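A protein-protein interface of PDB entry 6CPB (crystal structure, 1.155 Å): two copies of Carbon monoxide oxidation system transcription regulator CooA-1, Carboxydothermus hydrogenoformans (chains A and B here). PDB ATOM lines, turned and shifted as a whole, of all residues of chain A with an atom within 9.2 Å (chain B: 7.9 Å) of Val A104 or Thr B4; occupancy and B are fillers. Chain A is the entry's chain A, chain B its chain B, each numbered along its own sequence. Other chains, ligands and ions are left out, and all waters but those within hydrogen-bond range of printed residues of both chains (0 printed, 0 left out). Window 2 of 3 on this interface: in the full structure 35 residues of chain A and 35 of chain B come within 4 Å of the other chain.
The backbone carbonyl oxygen (O) of Pro A107 sits at hydrogen-bond distance from the side-chain hydroxyl (OG) of Ser A110 (2.6 Å).
O of Pro B107 is in hydrogen-bond range of OG of Ser B110 (3.0 Å).
Of the 15 printed residues of chain A, 4 touch a printed residue of chain B.
Hydrophobic or aromatic side chains of chain A that line the printed part of chain B: Val A103, Val A104 and Pro A107.
Hydrophobic or aromatic side chains of chain B that line the printed part of chain A: Val B103, Pro B107 and Leu B111.
Among the printed residues, 8 pairs touch across the chains.
Val A104 touches just these residues of chain B: Thr B4 (3.3 Å) and Pro B107 (3.6 Å).
Printed residues of chain B within 4 Å of Ser A110: Val B103 and Ser B110.
Thr B4 touches just one residue of chain A: Val A104.
Of the printed residues of chain A, Val B103 touches Pro A107 and Ser A110.
Printed residues of chain A within 4 Å of Pro B107: Val A103 and Val A104.
Printed residues of chain A within 4 Å of Ser B110: Ser A110 (2.7 Å).
Among the printed residues, merely in contact across the chains: Val A103 with Pro B107, Val A103 with Leu B111, Val A104 with Thr B4, Val A104 with Pro B107, Pro A107 with Val B103, Pro A107 with Val B104 and Ser A110 with Val B103.
Val A103 touches Pro B107, and with the chains exchanged Pro A107 touches Val B103.
Val A104 touches Pro B107, and with the chains exchanged Pro A107 touches Val B104.
Ser A110 touches Val B103, but with the chains exchanged Val A103 does not touch Ser B110 (4.3 Å).
Ser B110 touches its own counterpart, Ser A110.
Positions printed for both chains: 103, 104, 105, 106, 107, 108, 109 and 110.
OG of Ser A110 sits at hydrogen-bond distance from OG of Ser B110, 2.7 Å away.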
ATOM      1  N   VAL A  20      15.366  40.495 -18.263  1.00  0.00           N
ATOM      2  CA  VAL A  20      14.299  39.509 -18.296  1.00  0.00           C
ATOM      3  C   VAL A  20      13.577  39.449 -16.954  1.00  0.00           C
ATOM      4  O   VAL A  20      12.365  39.218 -16.906  1.00  0.00           O
ATOM      5  CB  VAL A  20      14.818  38.145 -18.788  1.00  0.00           C
ATOM      6  CG1 VAL A  20      15.779  37.532 -17.806  1.00  0.00           C
ATOM      7  CG2 VAL A  20      13.662  37.212 -19.078  1.00  0.00           C
ATOM      8  N   ARG A  97       2.813  31.099 -19.965  1.00  0.00           N
ATOM      9  CA  ARG A  97       3.226  31.256 -21.359  1.00  0.00           C
ATOM     10  C   ARG A  97       4.470  32.126 -21.464  1.00  0.00           C
ATOM     11  O   ARG A  97       5.401  31.822 -22.225  1.00  0.00           O
ATOM     12  CB  ARG A  97       2.096  31.880 -22.180  1.00  0.00           C
ATOM     13  CG  ARG A  97       0.927  30.961 -22.486  1.00  0.00           C
ATOM     14  CD  ARG A  97      -0.077  31.677 -23.384  1.00  0.00           C
ATOM     15  NE  ARG A  97      -1.274  30.880 -23.641  1.00  0.00           N
ATOM     16  CZ  ARG A  97      -1.390  29.979 -24.613  1.00  0.00           C
ATOM     17  NH1 ARG A  97      -0.377  29.737 -25.436  1.00  0.00           N
ATOM     18  NH2 ARG A  97      -2.526  29.311 -24.760  1.00  0.00           N
ATOM     19  N   ASN A  98       4.495  33.235 -20.734  1.00  0.00           N
ATOM     20  CA  ASN A  98       5.667  34.089 -20.771  1.00  0.00           C
ATOM     21  C   ASN A  98       6.882  33.352 -20.237  1.00  0.00           C
ATOM     22  O   ASN A  98       7.985  33.473 -20.783  1.00  0.00           O
ATOM     23  CB  ASN A  98       5.418  35.371 -19.989  1.00  0.00           C
ATOM     24  CG  ASN A  98       6.501  36.386 -20.214  1.00  0.00           C
ATOM     25  OD1 ASN A  98       6.895  36.656 -21.362  1.00  0.00           O
ATOM     26  ND2 ASN A  98       7.004  36.953 -19.135  1.00  0.00           N
ATOM     27  N   PHE A  99       6.702  32.596 -19.156  1.00  0.00           N
ATOM     28  CA  PHE A  99       7.811  31.823 -18.614  1.00  0.00           C
ATOM     29  C   PHE A  99       8.375  30.853 -19.646  1.00  0.00           C
ATOM     30  O   PHE A  99       9.593  30.713 -19.777  1.00  0.00           O
ATOM     31  CB  PHE A  99       7.385  31.068 -17.364  1.00  0.00           C
ATOM     32  CG  PHE A  99       8.507  30.309 -16.763  1.00  0.00           C
ATOM     33  CD1 PHE A  99       9.546  30.986 -16.142  1.00  0.00           C
ATOM     34  CD2 PHE A  99       8.584  28.939 -16.889  1.00  0.00           C
ATOM     35  CE1 PHE A  99      10.613  30.301 -15.607  1.00  0.00           C
ATOM     36  CE2 PHE A  99       9.663  28.240 -16.334  1.00  0.00           C
ATOM     37  CZ  PHE A  99      10.665  28.921 -15.697  1.00  0.00           C
ATOM     38  N   GLN A 100       7.506  30.143 -20.362  1.00  0.00           N
ATOM     39  CA  GLN A 100       7.988  29.203 -21.366  1.00  0.00           C
ATOM     40  C   GLN A 100       8.783  29.916 -22.454  1.00  0.00           C
ATOM     41  O   GLN A 100       9.801  29.400 -22.931  1.00  0.00           O
ATOM     42  CB  GLN A 100       6.806  28.407 -21.917  1.00  0.00           C
ATOM     43  CG  GLN A 100       6.229  27.441 -20.865  1.00  0.00           C
ATOM     44  CD  GLN A 100       4.885  26.854 -21.236  1.00  0.00           C
ATOM     45  OE1 GLN A 100       4.150  27.410 -22.052  1.00  0.00           O
ATOM     46  NE2 GLN A 100       4.554  25.725 -20.629  1.00  0.00           N
ATOM     47  N   ASN A 101       8.353  31.115 -22.848  1.00  0.00           N
ATOM     48  CA  ASN A 101       9.133  31.896 -23.799  1.00  0.00           C
ATOM     49  C   ASN A 101      10.478  32.317 -23.216  1.00  0.00           C
ATOM     50  O   ASN A 101      11.502  32.274 -23.910  1.00  0.00           O
ATOM     51  CB  ASN A 101       8.333  33.119 -24.246  1.00  0.00           C
ATOM     52  CG  ASN A 101       7.215  32.763 -25.199  1.00  0.00           C
ATOM     53  OD1 ASN A 101       7.335  31.829 -25.991  1.00  0.00           O
ATOM     54  ND2 ASN A 101       6.126  33.518 -25.143  1.00  0.00           N
ATOM     55  N   ILE A 102      10.495  32.738 -21.951  1.00  0.00           N
ATOM     56  CA  ILE A 102      11.746  33.074 -21.274  1.00  0.00           C
ATOM     57  C   ILE A 102      12.716  31.899 -21.292  1.00  0.00           C
ATOM     58  O   ILE A 102      13.914  32.071 -21.553  1.00  0.00           O
ATOM     59  CB  ILE A 102      11.453  33.549 -19.837  1.00  0.00           C
ATOM     60  CG1 ILE A 102      10.833  34.950 -19.856  1.00  0.00           C
ATOM     61  CG2 ILE A 102      12.717  33.505 -18.974  1.00  0.00           C
ATOM     62  CD1 ILE A 102      10.225  35.351 -18.536  1.00  0.00           C
ATOM     63  N   VAL A 103      12.221  30.689 -21.016  1.00  0.00           N
ATOM     64  CA  VAL A 103      13.086  29.514 -20.923  1.00  0.00           C
ATOM     65  C   VAL A 103      13.818  29.242 -22.230  1.00  0.00           C
ATOM     66  O   VAL A 103      14.948  28.736 -22.220  1.00  0.00           O
ATOM     67  CB  VAL A 103      12.248  28.297 -20.475  1.00  0.00           C
ATOM     68  CG1 VAL A 103      12.970  26.980 -20.722  1.00  0.00           C
ATOM     69  CG2 VAL A 103      11.900  28.406 -18.998  1.00  0.00           C
ATOM     70  N   VAL A 104      13.186  29.523 -23.373  1.00  0.00           N
ATOM     71  CA  VAL A 104      13.840  29.285 -24.656  1.00  0.00           C
ATOM     72  C   VAL A 104      15.140  30.068 -24.740  1.00  0.00           C
ATOM     73  O   VAL A 104      16.141  29.583 -25.279  1.00  0.00           O
ATOM     74  CB  VAL A 104      12.877  29.612 -25.813  1.00  0.00           C
ATOM     75  CG1 VAL A 104      13.603  29.548 -27.156  1.00  0.00           C
ATOM     76  CG2 VAL A 104      11.693  28.639 -25.801  1.00  0.00           C
ATOM     77  N   GLU A 105      15.142  31.291 -24.220  1.00  0.00           N
ATOM     78  CA  GLU A 105      16.328  32.138 -24.214  1.00  0.00           C
ATOM     79  C   GLU A 105      17.207  31.892 -22.991  1.00  0.00           C
ATOM     80  O   GLU A 105      18.441  31.933 -23.089  1.00  0.00           O
ATOM     81  CB  GLU A 105      15.896  33.608 -24.259  1.00  0.00           C
ATOM     82  CG  GLU A 105      17.033  34.622 -24.305  1.00  0.00           C
ATOM     83  CD  GLU A 105      17.835  34.556 -25.587  1.00  0.00           C
ATOM     84  OE1 GLU A 105      17.383  33.897 -26.547  1.00  0.00           O
ATOM     85  OE2 GLU A 105      18.916  35.177 -25.631  1.00  0.00           O
ATOM     86  N   PHE A 106      16.587  31.621 -21.844  1.00  0.00           N
ATOM     87  CA  PHE A 106      17.265  31.565 -20.547  1.00  0.00           C
ATOM     88  C   PHE A 106      16.867  30.274 -19.842  1.00  0.00           C
ATOM     89  O   PHE A 106      16.086  30.286 -18.882  1.00  0.00           O
ATOM     90  CB  PHE A 106      16.876  32.770 -19.684  1.00  0.00           C
ATOM     91  CG  PHE A 106      17.273  34.091 -20.264  1.00  0.00           C
ATOM     92  CD1 PHE A 106      18.578  34.523 -20.180  1.00  0.00           C
ATOM     93  CD2 PHE A 106      16.330  34.907 -20.872  1.00  0.00           C
ATOM     94  CE1 PHE A 106      18.945  35.756 -20.712  1.00  0.00           C
ATOM     95  CE2 PHE A 106      16.689  36.131 -21.391  1.00  0.00           C
ATOM     96  CZ  PHE A 106      17.998  36.544 -21.312  1.00  0.00           C
ATOM     97  N   PRO A 107      17.409  29.135 -20.277  1.00  0.00           N
ATOM     98  CA  PRO A 107      16.958  27.847 -19.730  1.00  0.00           C
ATOM     99  C   PRO A 107      17.358  27.585 -18.283  1.00  0.00           C
ATOM    100  O   PRO A 107      16.833  26.634 -17.690  1.00  0.00           O
ATOM    101  CB  PRO A 107      17.582  26.815 -20.681  1.00  0.00           C
ATOM    102  CG  PRO A 107      18.607  27.524 -21.413  1.00  0.00           C
ATOM    103  CD  PRO A 107      18.260  28.958 -21.457  1.00  0.00           C
ATOM    104  N   ALA A 108      18.243  28.379 -17.679  1.00  0.00           N
ATOM    105  CA  ALA A 108      18.599  28.144 -16.281  1.00  0.00           C
ATOM    106  C   ALA A 108      17.368  28.057 -15.379  1.00  0.00           C
ATOM    107  O   ALA A 108      17.320  27.228 -14.461  1.00  0.00           O
ATOM    108  CB  ALA A 108      19.533  29.242 -15.788  1.00  0.00           C
ATOM    109  N   PHE A 109      16.358  28.895 -15.623  1.00  0.00           N
ATOM    110  CA  PHE A 109      15.165  28.873 -14.787  1.00  0.00           C
ATOM    111  C   PHE A 109      14.524  27.494 -14.792  1.00  0.00           C
ATOM    112  O   PHE A 109      13.979  27.039 -13.775  1.00  0.00           O
ATOM    113  CB  PHE A 109      14.146  29.900 -15.286  1.00  0.00           C
ATOM    114  CG  PHE A 109      14.592  31.345 -15.166  1.00  0.00           C
ATOM    115  CD1 PHE A 109      14.507  32.017 -13.964  1.00  0.00           C
ATOM    116  CD2 PHE A 109      15.039  32.042 -16.269  1.00  0.00           C
ATOM    117  CE1 PHE A 109      14.893  33.342 -13.861  1.00  0.00           C
ATOM    118  CE2 PHE A 109      15.438  33.357 -16.171  1.00  0.00           C
ATOM    119  CZ  PHE A 109      15.356  34.012 -14.969  1.00  0.00           C
ATOM    120  N   SER A 110      14.567  26.817 -15.936  1.00  0.00           N
ATOM    121  CA  SER A 110      13.911  25.527 -16.048  1.00  0.00           C
ATOM    122  C   SER A 110      14.675  24.432 -15.329  1.00  0.00           C
ATOM    123  O   SER A 110      14.068  23.435 -14.926  1.00  0.00           O
ATOM    124  CB  SER A 110      13.742  25.159 -17.515  1.00  0.00           C
ATOM    125  OG  SER A 110      14.983  24.806 -18.137  1.00  0.00           O
ATOM    126  N   THR B   4      10.165  26.784 -31.084  1.00  0.00           N
ATOM    127  CA  THR B   4      11.046  25.733 -30.586  1.00  0.00           C
ATOM    128  C   THR B   4      10.493  24.357 -30.941  1.00  0.00           C
ATOM    129  O   THR B   4       9.313  24.077 -30.731  1.00  0.00           O
ATOM    130  CB  THR B   4      11.220  25.824 -29.056  1.00  0.00           C
ATOM    131  OG1 THR B   4      11.762  27.105 -28.713  1.00  0.00           O
ATOM    132  CG2 THR B   4      12.154  24.732 -28.544  1.00  0.00           C
ATOM    133  N   ASP B   5      11.358  23.498 -31.473  1.00  0.00           N
ATOM    134  CA  ASP B   5      10.978  22.133 -31.828  1.00  0.00           C
ATOM    135  C   ASP B   5      10.989  21.271 -30.568  1.00  0.00           C
ATOM    136  O   ASP B   5      12.049  21.042 -29.974  1.00  0.00           O
ATOM    137  CB  ASP B   5      11.951  21.588 -32.866  1.00  0.00           C
ATOM    138  CG  ASP B   5      11.515  20.254 -33.438  1.00  0.00           C
ATOM    139  OD1 ASP B   5      10.553  19.658 -32.915  1.00  0.00           O
ATOM    140  OD2 ASP B   5      12.138  19.806 -34.426  1.00  0.00           O
ATOM    141  N   THR B   6       9.814  20.786 -30.162  1.00  0.00           N
ATOM    142  CA  THR B   6       9.664  19.969 -28.961  1.00  0.00           C
ATOM    143  C   THR B   6       9.511  18.478 -29.264  1.00  0.00           C
ATOM    144  O   THR B   6       9.268  17.683 -28.346  1.00  0.00           O
ATOM    145  CB  THR B   6       8.468  20.459 -28.148  1.00  0.00           C
ATOM    146  OG1 THR B   6       7.276  20.301 -28.923  1.00  0.00           O
ATOM    147  CG2 THR B   6       8.641  21.929 -27.782  1.00  0.00           C
ATOM    148  N   ASN B   7       9.637  18.085 -30.527  1.00  0.00           N
ATOM    149  CA  ASN B   7       9.749  16.676 -30.905  1.00  0.00           C
ATOM    150  C   ASN B   7      11.200  16.289 -30.649  1.00  0.00           C
ATOM    151  O   ASN B   7      12.080  16.500 -31.489  1.00  0.00           O
ATOM    152  CB  ASN B   7       9.363  16.513 -32.369  1.00  0.00           C
ATOM    153  CG  ASN B   7       9.386  15.078 -32.832  1.00  0.00           C
ATOM    154  OD1 ASN B   7      10.080  14.239 -32.275  1.00  0.00           O
ATOM    155  ND2 ASN B   7       8.635  14.795 -33.886  1.00  0.00           N
ATOM    156  N   LEU B   8      11.465  15.757 -29.455  1.00  0.00           N
ATOM    157  CA  LEU B   8      12.849  15.567 -29.029  1.00  0.00           C
ATOM    158  C   LEU B   8      13.575  14.544 -29.891  1.00  0.00           C
ATOM    159  O   LEU B   8      14.775  14.695 -30.154  1.00  0.00           O
ATOM    160  CB  LEU B   8      12.914  15.179 -27.559  1.00  0.00           C
ATOM    161  CG  LEU B   8      12.287  16.153 -26.565  1.00  0.00           C
ATOM    162  CD1 LEU B   8      12.409  15.597 -25.159  1.00  0.00           C
ATOM    163  CD2 LEU B   8      12.923  17.553 -26.649  1.00  0.00           C
ATOM    164  N   VAL B  11      14.715  16.295 -32.971  1.00  0.00           N
ATOM    165  CA  VAL B  11      15.872  17.137 -32.683  1.00  0.00           C
ATOM    166  C   VAL B  11      17.141  16.299 -32.651  1.00  0.00           C
ATOM    167  O   VAL B  11      18.163  16.657 -33.249  1.00  0.00           O
ATOM    168  CB  VAL B  11      15.671  17.902 -31.364  1.00  0.00           C
ATOM    169  CG1 VAL B  11      16.955  18.627 -30.956  1.00  0.00           C
ATOM    170  CG2 VAL B  11      14.503  18.883 -31.479  1.00  0.00           C
ATOM    171  N   VAL B 103      20.258  20.724 -21.656  1.00  0.00           N
ATOM    172  CA  VAL B 103      19.157  21.679 -21.537  1.00  0.00           C
ATOM    173  C   VAL B 103      19.607  23.089 -21.845  1.00  0.00           C
ATOM    174  O   VAL B 103      18.869  23.861 -22.468  1.00  0.00           O
ATOM    175  CB  VAL B 103      18.551  21.591 -20.128  1.00  0.00           C
ATOM    176  CG1 VAL B 103      17.695  22.822 -19.810  1.00  0.00           C
ATOM    177  CG2 VAL B 103      17.728  20.324 -20.015  1.00  0.00           C
ATOM    178  N   VAL B 104      20.799  23.474 -21.381  1.00  0.00           N
ATOM    179  CA  VAL B 104      21.184  24.860 -21.552  1.00  0.00           C
ATOM    180  C   VAL B 104      21.396  25.160 -23.030  1.00  0.00           C
ATOM    181  O   VAL B 104      21.408  26.330 -23.426  1.00  0.00           O
ATOM    182  CB  VAL B 104      22.379  25.277 -20.658  1.00  0.00           C
ATOM    183  CG1 VAL B 104      22.019  25.186 -19.189  1.00  0.00           C
ATOM    184  CG2 VAL B 104      23.632  24.482 -20.983  1.00  0.00           C
ATOM    185  N   GLU B 105      21.578  24.129 -23.863  1.00  0.00           N
ATOM    186  CA  GLU B 105      21.665  24.257 -25.315  1.00  0.00           C
ATOM    187  C   GLU B 105      20.362  23.961 -26.049  1.00  0.00           C
ATOM    188  O   GLU B 105      20.111  24.530 -27.117  1.00  0.00           O
ATOM    189  CB  GLU B 105      22.759  23.319 -25.845  1.00  0.00           C
ATOM    190  CG  GLU B 105      24.126  23.677 -25.338  1.00  0.00           C
ATOM    191  CD  GLU B 105      24.475  25.072 -25.760  1.00  0.00           C
ATOM    192  OE1 GLU B 105      24.644  25.949 -24.893  1.00  0.00           O
ATOM    193  OE2 GLU B 105      24.540  25.296 -26.988  1.00  0.00           O
ATOM    194  N   PHE B 106      19.544  23.066 -25.514  1.00  0.00           N
ATOM    195  CA  PHE B 106      18.294  22.615 -26.135  1.00  0.00           C
ATOM    196  C   PHE B 106      17.191  22.652 -25.084  1.00  0.00           C
ATOM    197  O   PHE B 106      16.824  21.613 -24.508  1.00  0.00           O
ATOM    198  CB  PHE B 106      18.443  21.201 -26.707  1.00  0.00           C
ATOM    199  CG  PHE B 106      19.457  21.108 -27.817  1.00  0.00           C
ATOM    200  CD1 PHE B 106      19.095  21.401 -29.118  1.00  0.00           C
ATOM    201  CD2 PHE B 106      20.769  20.764 -27.557  1.00  0.00           C
ATOM    202  CE1 PHE B 106      20.024  21.345 -30.150  1.00  0.00           C
ATOM    203  CE2 PHE B 106      21.699  20.695 -28.576  1.00  0.00           C
ATOM    204  CZ  PHE B 106      21.323  20.999 -29.876  1.00  0.00           C
ATOM    205  N   PRO B 107      16.639  23.838 -24.805  1.00  0.00           N
ATOM    206  CA  PRO B 107      15.640  23.962 -23.728  1.00  0.00           C
ATOM    207  C   PRO B 107      14.391  23.128 -23.926  1.00  0.00           C
ATOM    208  O   PRO B 107      13.671  22.895 -22.950  1.00  0.00           O
ATOM    209  CB  PRO B 107      15.308  25.457 -23.714  1.00  0.00           C
ATOM    210  CG  PRO B 107      16.384  26.117 -24.474  1.00  0.00           C
ATOM    211  CD  PRO B 107      17.048  25.139 -25.353  1.00  0.00           C
ATOM    212  N   ALA B 108      14.090  22.672 -25.139  1.00  0.00           N
ATOM    213  CA  ALA B 108      12.927  21.809 -25.313  1.00  0.00           C
ATOM    214  C   ALA B 108      12.997  20.593 -24.404  1.00  0.00           C
ATOM    215  O   ALA B 108      11.959  20.080 -23.969  1.00  0.00           O
ATOM    216  CB  ALA B 108      12.814  21.355 -26.765  1.00  0.00           C
ATOM    217  N   PHE B 109      14.197  20.103 -24.110  1.00  0.00           N
ATOM    218  CA  PHE B 109      14.308  18.942 -23.231  1.00  0.00           C
ATOM    219  C   PHE B 109      13.769  19.231 -21.834  1.00  0.00           C
ATOM    220  O   PHE B 109      13.128  18.372 -21.224  1.00  0.00           O
ATOM    221  CB  PHE B 109      15.753  18.455 -23.165  1.00  0.00           C
ATOM    222  CG  PHE B 109      16.174  17.690 -24.384  1.00  0.00           C
ATOM    223  CD1 PHE B 109      16.655  18.357 -25.501  1.00  0.00           C
ATOM    224  CD2 PHE B 109      16.078  16.309 -24.431  1.00  0.00           C
ATOM    225  CE1 PHE B 109      17.032  17.662 -26.630  1.00  0.00           C
ATOM    226  CE2 PHE B 109      16.459  15.617 -25.557  1.00  0.00           C
ATOM    227  CZ  PHE B 109      16.935  16.298 -26.661  1.00  0.00           C
ATOM    228  N   SER B 110      14.048  20.415 -21.289  1.00  0.00           N
ATOM    229  CA  SER B 110      13.533  20.725 -19.965  1.00  0.00           C
ATOM    230  C   SER B 110      12.067  21.135 -20.010  1.00  0.00           C
ATOM    231  O   SER B 110      11.335  20.863 -19.055  1.00  0.00           O
ATOM    232  CB  SER B 110      14.383  21.791 -19.289  1.00  0.00           C
ATOM    233  OG  SER B 110      14.321  22.998 -20.001  1.00  0.00           O
ATOM    234  N   LEU B 111      11.620  21.799 -21.078  1.00  0.00           N
ATOM    235  CA  LEU B 111      10.203  22.119 -21.182  1.00  0.00           C
ATOM    236  C   LEU B 111       9.366  20.844 -21.173  1.00  0.00           C
ATOM    237  O   LEU B 111       8.340  20.765 -20.486  1.00  0.00           O
ATOM    238  CB  LEU B 111       9.944  22.972 -22.428  1.00  0.00           C
ATOM    239  CG  LEU B 111      10.504  24.406 -22.373  1.00  0.00           C
ATOM    240  CD1 LEU B 111      10.656  25.018 -23.768  1.00  0.00           C
ATOM    241  CD2 LEU B 111       9.627  25.292 -21.497  1.00  0.00           C
ATOM    242  N   ASN B 112       9.816  19.818 -21.893  1.00  0.00           N
ATOM    243  CA  ASN B 112       9.092  18.559 -21.868  1.00  0.00           C
ATOM    244  C   ASN B 112       9.177  17.898 -20.495  1.00  0.00           C
ATOM    245  O   ASN B 112       8.171  17.391 -19.988  1.00  0.00           O
ATOM    246  CB  ASN B 112       9.621  17.647 -22.967  1.00  0.00           C
ATOM    247  CG  ASN B 112       9.169  18.079 -24.348  1.00  0.00           C
ATOM    248  OD1 ASN B 112       8.857  19.248 -24.606  1.00  0.00           O
ATOM    249  ND2 ASN B 112       9.134  17.128 -25.247  1.00  0.00           N
